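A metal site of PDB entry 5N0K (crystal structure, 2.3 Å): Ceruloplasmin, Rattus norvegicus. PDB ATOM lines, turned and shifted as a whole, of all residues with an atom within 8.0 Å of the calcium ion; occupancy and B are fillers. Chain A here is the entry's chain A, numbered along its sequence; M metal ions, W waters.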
ATOM      1  N   TYR A 126     -18.998  -8.736  -0.225  1.00  0.00           N
ATOM      2  CA  TYR A 126     -19.943  -9.606   0.472  1.00  0.00           C
ATOM      3  C   TYR A 126     -20.590  -8.774   1.580  1.00  0.00           C
ATOM      4  O   TYR A 126     -19.968  -7.860   2.117  1.00  0.00           O
ATOM      5  CB  TYR A 126     -19.227 -10.810   1.114  1.00  0.00           C
ATOM      6  CG  TYR A 126     -17.882 -10.495   1.780  1.00  0.00           C
ATOM      7  CD1 TYR A 126     -17.798  -9.990   3.071  1.00  0.00           C
ATOM      8  CD2 TYR A 126     -16.693 -10.682   1.083  1.00  0.00           C
ATOM      9  CE1 TYR A 126     -16.567  -9.689   3.640  1.00  0.00           C
ATOM     10  CE2 TYR A 126     -15.471 -10.387   1.643  1.00  0.00           C
ATOM     11  CZ  TYR A 126     -15.400  -9.902   2.915  1.00  0.00           C
ATOM     12  OH  TYR A 126     -14.159  -9.604   3.443  1.00  0.00           O
ATOM     13  N   THR A 127     -21.824  -9.100   1.928  1.00  0.00           N
ATOM     14  CA  THR A 127     -22.486  -8.494   3.101  1.00  0.00           C
ATOM     15  C   THR A 127     -21.963  -9.209   4.321  1.00  0.00           C
ATOM     16  O   THR A 127     -21.233 -10.206   4.204  1.00  0.00           O
ATOM     17  CB  THR A 127     -24.026  -8.628   3.008  1.00  0.00           C
ATOM     18  OG1 THR A 127     -24.372 -10.020   2.809  1.00  0.00           O
ATOM     19  CG2 THR A 127     -24.554  -7.787   1.877  1.00  0.00           C
ATOM     20  N   LYS A 128     -22.366  -8.737   5.497  1.00  0.00           N
ATOM     21  CA  LYS A 128     -21.979  -9.416   6.743  1.00  0.00           C
ATOM     22  C   LYS A 128     -22.466 -10.867   6.853  1.00  0.00           C
ATOM     23  O   LYS A 128     -21.826 -11.685   7.528  1.00  0.00           O
ATOM     24  CB  LYS A 128     -22.454  -8.616   7.952  1.00  0.00           C
ATOM     25  CG  LYS A 128     -21.638  -7.375   8.250  1.00  0.00           C
ATOM     26  CD  LYS A 128     -20.180  -7.662   8.621  1.00  0.00           C
ATOM     27  CE  LYS A 128     -20.006  -8.470   9.893  1.00  0.00           C
ATOM     28  NZ  LYS A 128     -18.553  -8.644  10.182  1.00  0.00           N
ATOM     29  N   ALA A 129     -23.570 -11.193   6.169  1.00  0.00           N
ATOM     30  CA  ALA A 129     -24.072 -12.556   6.078  1.00  0.00           C
ATOM     31  C   ALA A 129     -23.284 -13.455   5.107  1.00  0.00           C
ATOM     32  O   ALA A 129     -23.572 -14.652   5.008  1.00  0.00           O
ATOM     33  CB  ALA A 129     -25.539 -12.506   5.652  1.00  0.00           C
ATOM     34  N   ASN A 130     -22.328 -12.883   4.363  1.00  0.00           N
ATOM     35  CA  ASN A 130     -21.616 -13.608   3.297  1.00  0.00           C
ATOM     36  C   ASN A 130     -20.087 -13.585   3.453  1.00  0.00           C
ATOM     37  O   ASN A 130     -19.352 -13.972   2.540  1.00  0.00           O
ATOM     38  CB  ASN A 130     -22.072 -13.081   1.921  1.00  0.00           C
ATOM     39  CG  ASN A 130     -23.561 -13.366   1.664  1.00  0.00           C
ATOM     40  OD1 ASN A 130     -24.436 -12.501   1.851  1.00  0.00           O
ATOM     41  ND2 ASN A 130     -23.858 -14.591   1.336  1.00  0.00           N
ATOM     42  N   GLU A 131     -19.613 -13.225   4.641  1.00  0.00           N
ATOM     43  CA  GLU A 131     -18.195 -13.043   4.929  1.00  0.00           C
ATOM     44  C   GLU A 131     -17.491 -14.348   5.292  1.00  0.00           C
ATOM     45  O   GLU A 131     -16.333 -14.532   4.961  1.00  0.00           O
ATOM     46  CB  GLU A 131     -18.076 -12.061   6.087  1.00  0.00           C
ATOM     47  CG  GLU A 131     -16.666 -11.826   6.616  1.00  0.00           C
ATOM     48  CD  GLU A 131     -16.596 -10.657   7.575  1.00  0.00           C
ATOM     49  OE1 GLU A 131     -17.628 -10.290   8.181  1.00  0.00           O
ATOM     50  OE2 GLU A 131     -15.498 -10.091   7.722  1.00  0.00           O
ATOM     51  N   GLY A 132     -18.146 -15.234   6.026  1.00  0.00           N
ATOM     52  CA  GLY A 132     -17.514 -16.483   6.438  1.00  0.00           C
ATOM     53  C   GLY A 132     -16.360 -16.313   7.410  1.00  0.00           C
ATOM     54  O   GLY A 132     -15.351 -17.001   7.325  1.00  0.00           O
ATOM     55  N   ALA A 133     -16.534 -15.378   8.340  1.00  0.00           N
ATOM     56  CA  ALA A 133     -15.537 -15.165   9.390  1.00  0.00           C
ATOM     57  C   ALA A 133     -16.228 -14.771  10.691  1.00  0.00           C
ATOM     58  O   ALA A 133     -17.152 -13.942  10.683  1.00  0.00           O
ATOM     59  CB  ALA A 133     -14.534 -14.101   8.986  1.00  0.00           C
ATOM     60  N   ILE A 134     -15.757 -15.368  11.785  1.00  0.00           N
ATOM     61  CA  ILE A 134     -16.322 -15.131  13.084  1.00  0.00           C
ATOM     62  C   ILE A 134     -15.459 -14.215  13.966  1.00  0.00           C
ATOM     63  O   ILE A 134     -14.246 -14.432  14.173  1.00  0.00           O
ATOM     64  CB  ILE A 134     -16.631 -16.482  13.806  1.00  0.00           C
ATOM     65  CG1 ILE A 134     -17.788 -16.303  14.801  1.00  0.00           C
ATOM     66  CG2 ILE A 134     -15.375 -17.078  14.437  1.00  0.00           C
ATOM     67  CD1 ILE A 134     -18.554 -17.556  15.212  1.00  0.00           C
ATOM     68  N   TYR A 135     -16.101 -13.168  14.476  1.00  0.00           N
ATOM     69  CA  TYR A 135     -15.477 -12.227  15.375  1.00  0.00           C
ATOM     70  C   TYR A 135     -16.509 -11.275  15.901  1.00  0.00           C
ATOM     71  O   TYR A 135     -17.587 -11.158  15.308  1.00  0.00           O
ATOM     72  CB  TYR A 135     -14.405 -11.401  14.655  1.00  0.00           C
ATOM     73  CG  TYR A 135     -14.764 -10.686  13.355  1.00  0.00           C
ATOM     74  CD1 TYR A 135     -14.585 -11.302  12.127  1.00  0.00           C
ATOM     75  CD2 TYR A 135     -15.155  -9.354  13.368  1.00  0.00           C
ATOM     76  CE1 TYR A 135     -14.866 -10.625  10.940  1.00  0.00           C
ATOM     77  CE2 TYR A 135     -15.411  -8.659  12.178  1.00  0.00           C
ATOM     78  CZ  TYR A 135     -15.269  -9.304  10.984  1.00  0.00           C
ATOM     79  OH  TYR A 135     -15.520  -8.608   9.844  1.00  0.00           O
ATOM     80  N   ASP A 137     -18.653  -8.482  16.000  1.00  0.00           N
ATOM     81  CA  ASP A 137     -19.085  -7.539  14.937  1.00  0.00           C
ATOM     82  C   ASP A 137     -20.514  -6.959  15.101  1.00  0.00           C
ATOM     83  O   ASP A 137     -21.061  -6.388  14.138  1.00  0.00           O
ATOM     84  CB  ASP A 137     -18.962  -8.223  13.565  1.00  0.00           C
ATOM     85  CG  ASP A 137     -19.734  -9.521  13.483  1.00  0.00           C
ATOM     86  OD1 ASP A 137     -20.513  -9.770  14.432  1.00  0.00           O
ATOM     87  OD2 ASP A 137     -19.546 -10.295  12.508  1.00  0.00           O
ATOM     88  N   THR A 139     -23.184  -8.467  14.989  1.00  0.00           N
ATOM     89  CA  THR A 139     -24.154  -9.219  14.197  1.00  0.00           C
ATOM     90  C   THR A 139     -24.877 -10.298  15.063  1.00  0.00           C
ATOM     91  O   THR A 139     -24.394 -10.711  16.121  1.00  0.00           O
ATOM     92  CB  THR A 139     -23.522  -9.867  12.947  1.00  0.00           C
ATOM     93  OG1 THR A 139     -22.559 -10.877  13.306  1.00  0.00           O
ATOM     94  CG2 THR A 139     -22.866  -8.822  12.039  1.00  0.00           C
ATOM     95  N   THR A 140     -26.033 -10.723  14.578  1.00  0.00           N
ATOM     96  CA  THR A 140     -26.900 -11.661  15.307  1.00  0.00           C
ATOM     97  C   THR A 140     -27.446 -12.703  14.350  1.00  0.00           C
ATOM     98  O   THR A 140     -27.916 -12.342  13.291  1.00  0.00           O
ATOM     99  CB  THR A 140     -28.092 -10.935  16.016  1.00  0.00           C
ATOM    100  OG1 THR A 140     -27.589 -10.000  17.000  1.00  0.00           O
ATOM    101  CG2 THR A 140     -29.036 -11.904  16.744  1.00  0.00           C
ATOM    102  N   ASP A 141     -27.333 -13.977  14.731  1.00  0.00           N
ATOM    103  CA  ASP A 141     -28.144 -15.076  14.197  1.00  0.00           C
ATOM    104  C   ASP A 141     -28.234 -15.150  12.669  1.00  0.00           C
ATOM    105  O   ASP A 141     -27.488 -15.908  12.072  1.00  0.00           O
ATOM    106  CB  ASP A 141     -29.561 -15.047  14.833  1.00  0.00           C
ATOM    107  CG  ASP A 141     -29.547 -15.174  16.363  1.00  0.00           C
ATOM    108  OD1 ASP A 141     -28.655 -15.865  16.917  1.00  0.00           O
ATOM    109  OD2 ASP A 141     -30.435 -14.571  17.009  1.00  0.00           O
ATOM    110  N   PHE A 142     -29.125 -14.369  12.053  1.00  0.00           N
ATOM    111  CA  PHE A 142     -29.384 -14.371  10.583  1.00  0.00           C
ATOM    112  C   PHE A 142     -28.192 -13.928   9.694  1.00  0.00           C
ATOM    113  O   PHE A 142     -28.351 -13.621   8.529  1.00  0.00           O
ATOM    114  CB  PHE A 142     -30.723 -13.594  10.231  1.00  0.00           C
ATOM    115  CG  PHE A 142     -30.713 -12.048  10.415  1.00  0.00           C
ATOM    116  CD1 PHE A 142     -29.828 -11.373  11.269  1.00  0.00           C
ATOM    117  CD2 PHE A 142     -31.668 -11.258   9.737  1.00  0.00           C
ATOM    118  CE1 PHE A 142     -29.855  -9.987  11.431  1.00  0.00           C
ATOM    119  CE2 PHE A 142     -31.702  -9.865   9.889  1.00  0.00           C
ATOM    120  CZ  PHE A 142     -30.801  -9.227  10.742  1.00  0.00           C
ATOM    121  N   GLN A 143     -26.994 -14.081  10.244  1.00  0.00           N
ATOM    122  CA  GLN A 143     -25.825 -13.271   9.895  1.00  0.00           C
ATOM    123  C   GLN A 143     -24.556 -13.924  10.405  1.00  0.00           C
ATOM    124  O   GLN A 143     -23.491 -13.598   9.904  1.00  0.00           O
ATOM    125  CB  GLN A 143     -25.877 -11.858  10.502  1.00  0.00           C
ATOM    126  CG  GLN A 143     -26.411 -10.742   9.619  1.00  0.00           C
ATOM    127  CD  GLN A 143     -26.458  -9.383  10.347  1.00  0.00           C
ATOM    128  OE1 GLN A 143     -26.631  -9.305  11.583  1.00  0.00           O
ATOM    129  NE2 GLN A 143     -26.315  -8.308   9.588  1.00  0.00           N
ATOM    130  N   ARG A 144     -24.676 -14.743  11.449  1.00  0.00           N
ATOM    131  CA  ARG A 144     -23.590 -15.574  11.942  1.00  0.00           C
ATOM    132  C   ARG A 144     -23.646 -16.996  11.418  1.00  0.00           C
ATOM    133  O   ARG A 144     -22.853 -17.825  11.864  1.00  0.00           O
ATOM    134  CB  ARG A 144     -23.615 -15.581  13.465  1.00  0.00           C
ATOM    135  CG  ARG A 144     -22.994 -14.341  14.088  1.00  0.00           C
ATOM    136  CD  ARG A 144     -21.552 -14.617  14.501  1.00  0.00           C
ATOM    137  NE  ARG A 144     -20.894 -13.402  14.969  1.00  0.00           N
ATOM    138  CZ  ARG A 144     -21.104 -12.818  16.161  1.00  0.00           C
ATOM    139  NH1 ARG A 144     -21.980 -13.305  17.045  1.00  0.00           N
ATOM    140  NH2 ARG A 144     -20.427 -11.713  16.458  1.00  0.00           N
ATOM    141  N   ALA A 145     -24.528 -17.281  10.467  1.00  0.00           N
ATOM    142  CA  ALA A 145     -24.682 -18.650   9.953  1.00  0.00           C
ATOM    143  C   ALA A 145     -23.580 -18.991   8.967  1.00  0.00           C
ATOM    144  O   ALA A 145     -23.127 -20.141   8.914  1.00  0.00           O
ATOM    145  CB  ALA A 145     -26.050 -18.810   9.307  1.00  0.00           C
ATOM    146  N   ASP A 146     -23.187 -17.993   8.170  1.00  0.00           N
ATOM    147  CA  ASP A 146     -21.932 -18.030   7.383  1.00  0.00           C
ATOM    148  C   ASP A 146     -20.628 -18.242   8.143  1.00  0.00           C
ATOM    149  O   ASP A 146     -19.657 -18.742   7.566  1.00  0.00           O
ATOM    150  CB  ASP A 146     -21.771 -16.729   6.578  1.00  0.00           C
ATOM    151  CG  ASP A 146     -21.715 -15.504   7.457  1.00  0.00           C
ATOM    152  OD1 ASP A 146     -22.392 -15.538   8.482  1.00  0.00           O
ATOM    153  OD2 ASP A 146     -21.014 -14.502   7.159  1.00  0.00           O
ATOM    154  N   ASP A 147     -20.605 -17.879   9.422  1.00  0.00           N
ATOM    155  CA  ASP A 147     -19.366 -17.758  10.194  1.00  0.00           C
ATOM    156  C   ASP A 147     -18.827 -19.049  10.798  1.00  0.00           C
ATOM    157  O   ASP A 147     -17.674 -19.100  11.190  1.00  0.00           O
ATOM    158  CB  ASP A 147     -19.572 -16.670  11.257  1.00  0.00           C
ATOM    159  CG  ASP A 147     -19.979 -15.344  10.618  1.00  0.00           C
ATOM    160  OD1 ASP A 147     -19.751 -15.150   9.410  1.00  0.00           O
ATOM    161  OD2 ASP A 147     -20.513 -14.452  11.298  1.00  0.00           O
ATOM    162  N   LYS A 148     -19.653 -20.097  10.830  1.00  0.00           N
ATOM    163  CA  LYS A 148     -19.274 -21.415  11.392  1.00  0.00           C
ATOM    164  C   LYS A 148     -20.163 -22.512  10.747  1.00  0.00           C
ATOM    165  O   LYS A 148     -21.367 -22.512  10.935  1.00  0.00           O
ATOM    166  CB  LYS A 148     -19.452 -21.397  12.932  1.00  0.00           C
ATOM    167  CG  LYS A 148     -18.252 -21.907  13.709  1.00  0.00           C
ATOM    168  CD  LYS A 148     -18.534 -22.168  15.185  1.00  0.00           C
ATOM    169  CE  LYS A 148     -19.346 -21.068  15.844  1.00  0.00           C
ATOM    170  NZ  LYS A 148     -19.310 -21.165  17.331  1.00  0.00           N
ATOM    171  N   TYR A 155     -23.766 -23.979   3.211  1.00  0.00           N
ATOM    172  CA  TYR A 155     -24.082 -22.566   3.003  1.00  0.00           C
ATOM    173  C   TYR A 155     -23.787 -22.068   1.612  1.00  0.00           C
ATOM    174  O   TYR A 155     -22.824 -22.505   0.945  1.00  0.00           O
ATOM    175  CB  TYR A 155     -23.281 -21.687   3.963  1.00  0.00           C
ATOM    176  CG  TYR A 155     -23.924 -20.347   4.287  1.00  0.00           C
ATOM    177  CD1 TYR A 155     -23.568 -19.173   3.613  1.00  0.00           C
ATOM    178  CD2 TYR A 155     -24.877 -20.257   5.301  1.00  0.00           C
ATOM    179  CE1 TYR A 155     -24.144 -17.958   3.951  1.00  0.00           C
ATOM    180  CE2 TYR A 155     -25.450 -19.050   5.618  1.00  0.00           C
ATOM    181  CZ  TYR A 155     -25.082 -17.907   4.963  1.00  0.00           C
ATOM    182  OH  TYR A 155     -25.681 -16.759   5.325  1.00  0.00           O
ATOM    183  N   TYR A 157     -22.703 -18.864  -0.136  1.00  0.00           N
ATOM    184  CA  TYR A 157     -22.009 -17.570  -0.096  1.00  0.00           C
ATOM    185  C   TYR A 157     -22.189 -16.740  -1.387  1.00  0.00           C
ATOM    186  O   TYR A 157     -21.806 -17.170  -2.481  1.00  0.00           O
ATOM    187  CB  TYR A 157     -20.523 -17.816   0.140  1.00  0.00           C
ATOM    188  CG  TYR A 157     -20.174 -18.441   1.480  1.00  0.00           C
ATOM    189  CD1 TYR A 157     -20.090 -19.833   1.644  1.00  0.00           C
ATOM    190  CD2 TYR A 157     -19.880 -17.626   2.580  1.00  0.00           C
ATOM    191  CE1 TYR A 157     -19.750 -20.396   2.873  1.00  0.00           C
ATOM    192  CE2 TYR A 157     -19.551 -18.174   3.810  1.00  0.00           C
ATOM    193  CZ  TYR A 157     -19.467 -19.551   3.954  1.00  0.00           C
ATOM    194  OH  TYR A 157     -19.107 -20.053   5.209  1.00  0.00           O
ATOM    195  N   TRP A1030     -16.131  -4.477  10.591  1.00  0.00           N
ATOM    196  CA  TRP A1030     -15.249  -5.308   9.769  1.00  0.00           C
ATOM    197  C   TRP A1030     -13.870  -5.508  10.409  1.00  0.00           C
ATOM    198  O   TRP A1030     -13.310  -4.563  10.923  1.00  0.00           O
ATOM    199  CB  TRP A1030     -15.052  -4.634   8.416  1.00  0.00           C
ATOM    200  CG  TRP A1030     -16.289  -4.434   7.629  1.00  0.00           C
ATOM    201  CD1 TRP A1030     -16.913  -3.252   7.399  1.00  0.00           C
ATOM    202  CD2 TRP A1030     -17.038  -5.427   6.915  1.00  0.00           C
ATOM    203  NE1 TRP A1030     -18.011  -3.431   6.612  1.00  0.00           N
ATOM    204  CE2 TRP A1030     -18.108  -4.760   6.292  1.00  0.00           C
ATOM    205  CE3 TRP A1030     -16.922  -6.812   6.774  1.00  0.00           C
ATOM    206  CZ2 TRP A1030     -19.068  -5.421   5.517  1.00  0.00           C
ATOM    207  CZ3 TRP A1030     -17.861  -7.469   5.996  1.00  0.00           C
ATOM    208  CH2 TRP A1030     -18.939  -6.772   5.384  1.00  0.00           C
HETATM  209 CA    CA M   1     -21.277 -13.271   9.172  1.00  0.00          CA
HETATM  210  O   HOH W   1     -21.310 -11.830  10.481  1.00  0.00           O
HETATM  211  O   HOH W   2     -18.838 -12.286   9.470  1.00  0.00           O
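The side-chain amino group of Lys 128 lies within salt-bridge range of the side-chain carboxylate of Glu 131 (2.8 Å).
NZ of Lys 128 lies within salt-bridge range of OD2 of Asp 137.
The side-chain amino group (NZ) of Lys 128 lies within hydrogen-bond range of the side-chain hydroxyl (OH) of Tyr 135, 3.1 Å away.
OE1 of Gln 143 sits at hydrogen-bond distance from N of Thr 140 (3.4 Å).
OD2 of Asp 146 sits close to N of Glu 131 (3.2 Å).
The side-chain carboxylate of Asp 146 sits close to the backbone NH of Asn 130, at 3.5 Å.
OH of Tyr 157 is in hydrogen-bond range of O of Asp 146 (2.8 Å).
The side-chain carboxylate (OD2) of Asp 147 sits close to the guanidinium group (NE) of Arg 144.
Water W1 bridges the side-chain carboxylate of Asp 137 (3.1 Å) and the side-chain hydroxyl of Thr 139 (3.2 Å).
Water W2 lies within hydrogen-bond range of O of Ala 133 (2.7 Å) and OE1 of Glu 131 (2.7 Å).
Within 4 Å of the calcium ion: Lys 128, Gln 143, Asp 146 and Asp 147.
The calcium ion is bound by water W1, at 1.9 Å.
O of Lys 128 is bound to the calcium ion, at 2.3 Å.
O of Gln 143 binds the calcium ion (2.4 Å).
OD2 of Asp 146 is bound to the calcium ion, at 2.4 Å.
The side-chain carboxylate (OD1) of Asp 147 is bound to the calcium ion, at 2.4 Å.
The calcium ion is bound by the side-chain carboxylate (OD2) of Asp 147 (2.5 Å).
OD1 of Asp 146 binds the calcium ion, 2.6 Å away.
The calcium ion is bound by water W2.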
